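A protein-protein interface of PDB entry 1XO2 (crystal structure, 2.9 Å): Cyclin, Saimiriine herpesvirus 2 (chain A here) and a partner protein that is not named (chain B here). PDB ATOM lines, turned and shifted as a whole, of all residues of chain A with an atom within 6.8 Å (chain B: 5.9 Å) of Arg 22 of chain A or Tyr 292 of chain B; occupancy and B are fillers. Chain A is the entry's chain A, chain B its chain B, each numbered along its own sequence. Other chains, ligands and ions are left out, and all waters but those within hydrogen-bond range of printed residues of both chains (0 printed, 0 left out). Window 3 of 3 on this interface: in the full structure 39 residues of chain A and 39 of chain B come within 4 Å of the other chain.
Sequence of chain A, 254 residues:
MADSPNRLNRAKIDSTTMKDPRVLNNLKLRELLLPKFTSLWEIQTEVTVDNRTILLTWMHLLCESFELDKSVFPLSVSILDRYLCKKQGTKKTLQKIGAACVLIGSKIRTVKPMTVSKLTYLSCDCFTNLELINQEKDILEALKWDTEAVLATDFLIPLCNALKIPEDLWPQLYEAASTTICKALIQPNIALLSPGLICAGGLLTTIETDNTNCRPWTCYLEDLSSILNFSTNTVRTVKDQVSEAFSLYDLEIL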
ATOM      1  N   THR A  17     -14.462 -12.647  31.316  1.00  0.00           N
ATOM      2  CA  THR A  17     -14.844 -13.114  29.990  1.00  0.00           C
ATOM      3  C   THR A  17     -15.195 -14.595  30.001  1.00  0.00           C
ATOM      4  O   THR A  17     -15.783 -15.127  29.050  1.00  0.00           O
ATOM      5  CB  THR A  17     -13.733 -12.814  28.952  1.00  0.00           C
ATOM      6  OG1 THR A  17     -12.643 -13.721  29.119  1.00  0.00           O
ATOM      7  CG2 THR A  17     -13.219 -11.395  29.143  1.00  0.00           C
ATOM      8  N   ASP A  20     -19.130 -13.957  32.973  1.00  0.00           N
ATOM      9  CA  ASP A  20     -19.872 -12.692  33.040  1.00  0.00           C
ATOM     10  C   ASP A  20     -20.731 -12.346  31.789  1.00  0.00           C
ATOM     11  O   ASP A  20     -21.651 -11.541  31.901  1.00  0.00           O
ATOM     12  CB  ASP A  20     -18.919 -11.517  33.349  1.00  0.00           C
ATOM     13  CG  ASP A  20     -18.785 -11.219  34.863  1.00  0.00           C
ATOM     14  OD1 ASP A  20     -17.963 -10.362  35.273  1.00  0.00           O
ATOM     15  OD2 ASP A  20     -19.513 -11.834  35.662  1.00  0.00           O
ATOM     16  N   PRO A  21     -20.460 -12.947  30.598  1.00  0.00           N
ATOM     17  CA  PRO A  21     -21.209 -12.683  29.350  1.00  0.00           C
ATOM     18  C   PRO A  21     -22.509 -13.435  29.065  1.00  0.00           C
ATOM     19  O   PRO A  21     -23.604 -13.043  29.468  1.00  0.00           O
ATOM     20  CB  PRO A  21     -20.190 -13.003  28.244  1.00  0.00           C
ATOM     21  CG  PRO A  21     -18.890 -12.964  28.917  1.00  0.00           C
ATOM     22  CD  PRO A  21     -19.175 -13.572  30.258  1.00  0.00           C
ATOM     23  N   ARG A  22     -22.333 -14.494  28.280  1.00  0.00           N
ATOM     24  CA  ARG A  22     -23.379 -15.407  27.814  1.00  0.00           C
ATOM     25  C   ARG A  22     -22.765 -16.799  27.746  1.00  0.00           C
ATOM     26  O   ARG A  22     -22.901 -17.518  26.753  1.00  0.00           O
ATOM     27  CB  ARG A  22     -23.851 -15.002  26.424  1.00  0.00           C
ATOM     28  CG  ARG A  22     -22.755 -14.383  25.571  1.00  0.00           C
ATOM     29  CD  ARG A  22     -21.965 -15.381  24.768  1.00  0.00           C
ATOM     30  NE  ARG A  22     -20.838 -14.705  24.124  1.00  0.00           N
ATOM     31  CZ  ARG A  22     -20.254 -15.107  22.997  1.00  0.00           C
ATOM     32  NH1 ARG A  22     -20.697 -16.192  22.367  1.00  0.00           N
ATOM     33  NH2 ARG A  22     -19.215 -14.442  22.511  1.00  0.00           N
ATOM     34  N   VAL A  23     -22.037 -17.132  28.808  1.00  0.00           N
ATOM     35  CA  VAL A  23     -21.396 -18.417  28.946  1.00  0.00           C
ATOM     36  C   VAL A  23     -22.516 -19.325  29.422  1.00  0.00           C
ATOM     37  O   VAL A  23     -22.508 -20.534  29.199  1.00  0.00           O
ATOM     38  CB  VAL A  23     -20.281 -18.342  30.012  1.00  0.00           C
ATOM     39  CG1 VAL A  23     -19.815 -19.739  30.397  1.00  0.00           C
ATOM     40  CG2 VAL A  23     -19.119 -17.525  29.477  1.00  0.00           C
ATOM     41  N   LEU A  24     -23.492 -18.710  30.070  1.00  0.00           N
ATOM     42  CA  LEU A  24     -24.634 -19.422  30.602  1.00  0.00           C
ATOM     43  C   LEU A  24     -25.427 -20.030  29.461  1.00  0.00           C
ATOM     44  O   LEU A  24     -25.784 -21.206  29.502  1.00  0.00           O
ATOM     45  CB  LEU A  24     -25.529 -18.464  31.384  1.00  0.00           C
ATOM     46  CG  LEU A  24     -26.032 -18.910  32.754  1.00  0.00           C
ATOM     47  CD1 LEU A  24     -27.138 -17.964  33.201  1.00  0.00           C
ATOM     48  CD2 LEU A  24     -26.538 -20.339  32.678  1.00  0.00           C
ATOM     49  N   ASN A  25     -25.707 -19.232  28.438  1.00  0.00           N
ATOM     50  CA  ASN A  25     -26.468 -19.747  27.310  1.00  0.00           C
ATOM     51  C   ASN A  25     -25.791 -20.985  26.753  1.00  0.00           C
ATOM     52  O   ASN A  25     -26.460 -21.960  26.404  1.00  0.00           O
ATOM     53  CB  ASN A  25     -26.591 -18.708  26.191  1.00  0.00           C
ATOM     54  CG  ASN A  25     -27.286 -17.453  26.640  1.00  0.00           C
ATOM     55  OD1 ASN A  25     -28.055 -17.468  27.599  1.00  0.00           O
ATOM     56  ND2 ASN A  25     -27.034 -16.355  25.936  1.00  0.00           N
ATOM     57  N   ASN A  26     -24.463 -20.934  26.674  1.00  0.00           N
ATOM     58  CA  ASN A  26     -23.690 -22.046  26.138  1.00  0.00           C
ATOM     59  C   ASN A  26     -23.674 -23.254  27.067  1.00  0.00           C
ATOM     60  O   ASN A  26     -23.698 -24.398  26.595  1.00  0.00           O
ATOM     61  CB  ASN A  26     -22.254 -21.600  25.803  1.00  0.00           C
ATOM     62  CG  ASN A  26     -22.187 -20.701  24.561  1.00  0.00           C
ATOM     63  OD1 ASN A  26     -22.935 -20.898  23.590  1.00  0.00           O
ATOM     64  ND2 ASN A  26     -21.281 -19.726  24.582  1.00  0.00           N
ATOM     65  N   LEU A  27     -23.632 -23.008  28.378  1.00  0.00           N
ATOM     66  CA  LEU A  27     -23.642 -24.099  29.351  1.00  0.00           C
ATOM     67  C   LEU A  27     -24.991 -24.812  29.269  1.00  0.00           C
ATOM     68  O   LEU A  27     -25.058 -26.042  29.295  1.00  0.00           O
ATOM     69  CB  LEU A  27     -23.420 -23.571  30.766  1.00  0.00           C
ATOM     70  CG  LEU A  27     -21.995 -23.651  31.322  1.00  0.00           C
ATOM     71  CD1 LEU A  27     -21.818 -22.745  32.526  1.00  0.00           C
ATOM     72  CD2 LEU A  27     -21.691 -25.080  31.669  1.00  0.00           C
ATOM     73  N   LEU B 130      -8.940 -14.423  16.461  1.00  0.00           N
ATOM     74  CA  LEU B 130      -9.768 -13.940  17.561  1.00  0.00           C
ATOM     75  C   LEU B 130     -11.134 -14.639  17.577  1.00  0.00           C
ATOM     76  O   LEU B 130     -11.835 -14.642  18.592  1.00  0.00           O
ATOM     77  CB  LEU B 130      -9.963 -12.425  17.456  1.00  0.00           C
ATOM     78  CG  LEU B 130      -8.722 -11.628  17.845  1.00  0.00           C
ATOM     79  CD1 LEU B 130      -8.926 -10.136  17.616  1.00  0.00           C
ATOM     80  CD2 LEU B 130      -8.422 -11.905  19.300  1.00  0.00           C
ATOM     81  N   ASP B 134     -12.716 -16.426  20.952  1.00  0.00           N
ATOM     82  CA  ASP B 134     -14.035 -16.028  21.446  1.00  0.00           C
ATOM     83  C   ASP B 134     -14.850 -17.283  21.680  1.00  0.00           C
ATOM     84  O   ASP B 134     -15.493 -17.415  22.712  1.00  0.00           O
ATOM     85  CB  ASP B 134     -14.767 -15.124  20.453  1.00  0.00           C
ATOM     86  CG  ASP B 134     -16.149 -14.700  20.961  1.00  0.00           C
ATOM     87  OD1 ASP B 134     -16.211 -13.984  21.969  1.00  0.00           O
ATOM     88  OD2 ASP B 134     -17.182 -15.081  20.368  1.00  0.00           O
ATOM     89  N   SER B 138     -15.894 -18.666  25.244  1.00  0.00           N
ATOM     90  CA  SER B 138     -17.335 -18.619  25.499  1.00  0.00           C
ATOM     91  C   SER B 138     -17.822 -19.941  26.096  1.00  0.00           C
ATOM     92  O   SER B 138     -18.932 -20.011  26.633  1.00  0.00           O
ATOM     93  CB  SER B 138     -18.123 -18.281  24.225  1.00  0.00           C
ATOM     94  OG  SER B 138     -18.100 -19.346  23.290  1.00  0.00           O
ATOM     95  N   SER B 290     -10.833  -8.401  25.752  1.00  0.00           N
ATOM     96  CA  SER B 290     -11.266  -9.782  25.546  1.00  0.00           C
ATOM     97  C   SER B 290     -11.489 -10.068  24.070  1.00  0.00           C
ATOM     98  O   SER B 290     -11.881  -9.181  23.310  1.00  0.00           O
ATOM     99  CB  SER B 290     -12.565 -10.057  26.290  1.00  0.00           C
ATOM    100  OG  SER B 290     -13.662  -9.492  25.605  1.00  0.00           O
ATOM    101  N   ALA B 291     -11.249 -11.318  23.681  1.00  0.00           N
ATOM    102  CA  ALA B 291     -11.422 -11.755  22.300  1.00  0.00           C
ATOM    103  C   ALA B 291     -12.793 -11.322  21.779  1.00  0.00           C
ATOM    104  O   ALA B 291     -12.959 -11.040  20.584  1.00  0.00           O
ATOM    105  CB  ALA B 291     -11.277 -13.272  22.211  1.00  0.00           C
ATOM    106  N   TYR B 292     -13.770 -11.269  22.680  1.00  0.00           N
ATOM    107  CA  TYR B 292     -15.109 -10.864  22.304  1.00  0.00           C
ATOM    108  C   TYR B 292     -15.035  -9.430  21.791  1.00  0.00           C
ATOM    109  O   TYR B 292     -15.147  -9.183  20.591  1.00  0.00           O
ATOM    110  CB  TYR B 292     -16.062 -10.957  23.506  1.00  0.00           C
ATOM    111  CG  TYR B 292     -17.523 -10.740  23.154  1.00  0.00           C
ATOM    112  CD1 TYR B 292     -18.035 -11.179  21.937  1.00  0.00           C
ATOM    113  CD2 TYR B 292     -18.385 -10.083  24.020  1.00  0.00           C
ATOM    114  CE1 TYR B 292     -19.360 -10.963  21.586  1.00  0.00           C
ATOM    115  CE2 TYR B 292     -19.728  -9.862  23.679  1.00  0.00           C
ATOM    116  CZ  TYR B 292     -20.203 -10.304  22.458  1.00  0.00           C
ATOM    117  OH  TYR B 292     -21.519 -10.097  22.092  1.00  0.00           O
ATOM    118  N   SER B 293     -14.829  -8.488  22.701  1.00  0.00           N
ATOM    119  CA  SER B 293     -14.743  -7.087  22.330  1.00  0.00           C
ATOM    120  C   SER B 293     -13.723  -6.842  21.218  1.00  0.00           C
ATOM    121  O   SER B 293     -13.882  -5.920  20.413  1.00  0.00           O
ATOM    122  CB  SER B 293     -14.388  -6.259  23.560  1.00  0.00           C
ATOM    123  OG  SER B 293     -13.173  -6.710  24.123  1.00  0.00           O
ATOM    124  N   ALA B 294     -12.679  -7.662  21.175  1.00  0.00           N
ATOM    125  CA  ALA B 294     -11.640  -7.519  20.156  1.00  0.00           C
ATOM    126  C   ALA B 294     -12.173  -7.632  18.716  1.00  0.00           C
ATOM    127  O   ALA B 294     -11.644  -6.988  17.801  1.00  0.00           O
ATOM    128  CB  ALA B 294     -10.540  -8.543  20.384  1.00  0.00           C
ATOM    129  N   LEU B 295     -13.201  -8.453  18.510  1.00  0.00           N
ATOM    130  CA  LEU B 295     -13.785  -8.624  17.182  1.00  0.00           C
ATOM    131  C   LEU B 295     -14.667  -7.429  16.841  1.00  0.00           C
ATOM    132  O   LEU B 295     -15.170  -7.342  15.729  1.00  0.00           O
ATOM    133  CB  LEU B 295     -14.636  -9.894  17.122  1.00  0.00           C
ATOM    134  CG  LEU B 295     -14.018 -11.283  17.339  1.00  0.00           C
ATOM    135  CD1 LEU B 295     -15.116 -12.276  17.690  1.00  0.00           C
ATOM    136  CD2 LEU B 295     -13.271 -11.733  16.093  1.00  0.00           C
ATOM    137  N   SER B 296     -14.865  -6.524  17.803  1.00  0.00           N
ATOM    138  CA  SER B 296     -15.681  -5.317  17.613  1.00  0.00           C
ATOM    139  C   SER B 296     -14.809  -4.100  17.357  1.00  0.00           C
ATOM    140  O   SER B 296     -15.262  -3.115  16.785  1.00  0.00           O
ATOM    141  CB  SER B 296     -16.530  -5.026  18.847  1.00  0.00           C
ATOM    142  OG  SER B 296     -17.589  -5.947  18.960  1.00  0.00           O
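The side-chain amide nitrogen (ND2) of Asn 26 of chain A sits at hydrogen-bond distance from the backbone carbonyl oxygen (O) of Arg 22 of chain A, 3.5 Å away. The backbone carbonyl oxygen (O) of Asp 134 of chain B sits close to the side-chain hydroxyl (OG) of Ser 138 of chain B (3.3 Å). The backbone NH of Tyr 292 of chain B lies close to the side-chain hydroxyl of Ser 290 of chain B. The side-chain hydroxyl (OG) of Ser 293 of chain B sits at hydrogen-bond distance from the backbone carbonyl oxygen (O) of Ser 290 of chain B (2.9 Å).
Hydrophobic or aromatic side chains of chain A within 4 Å of the printed part of chain B: Val 23. Along chain A the printed residues that touch a printed residue of chain B span positions 17 to 26. Of the 10 printed residues of chain B, 4 touch a printed residue of chain A. Hydrophobic or aromatic side chains of chain B that line the printed part of chain A: Tyr 292. Among the printed residues, 6 pairs touch across the chains. Among the printed residues, Asp or Glu carboxylates within 4 Å of a Lys or Arg side-chain nitrogen of the other chain: Arg 22 of chain A with Asp 134 of chain B.
Of the printed residues of chain B, Thr 17 of chain A touches Ser 290 (3.2 Å). Arg 22 of chain A touches three residues of chain B. Printed residues of chain B within 4 Å of Val 23 of chain A: Ser 138. Printed residues of chain A within 4 Å of Asp 134 of chain B: Arg 22 (3.0 Å). Of the printed residues of chain A, Ser 138 of chain B touches Arg 22, Val 23 and Asn 26. Of the printed residues of chain A, Ser 290 of chain B touches Thr 17. Ala 291 of chain B touches none of the printed residues of chain A. Ala 294 of chain B touches none of the printed residues of chain A. The nearest printed residue of chain B that does not touch Arg 22 of chain A is Leu 295 of chain B (6.7 Å).
ND2 of Asn 26 of chain A lies within hydrogen-bond range of O of Ser 138 of chain B (3.1 Å). The guanidinium group of Arg 22 of chain A lies within salt-bridge range of the side-chain carboxylate of Asp 134 of chain B, 3.0 Å away.
Among the printed residues, merely in contact across the chains: Thr 17 of chain A with Ser 290 of chain B (3.2 Å), Arg 22 of chain A with Tyr 292 of chain B (3.5 Å), Val 23 of chain A with Ser 138 of chain B (3.7 Å) and Arg 22 of chain A with Ser 138 of chain B (3.8 Å).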
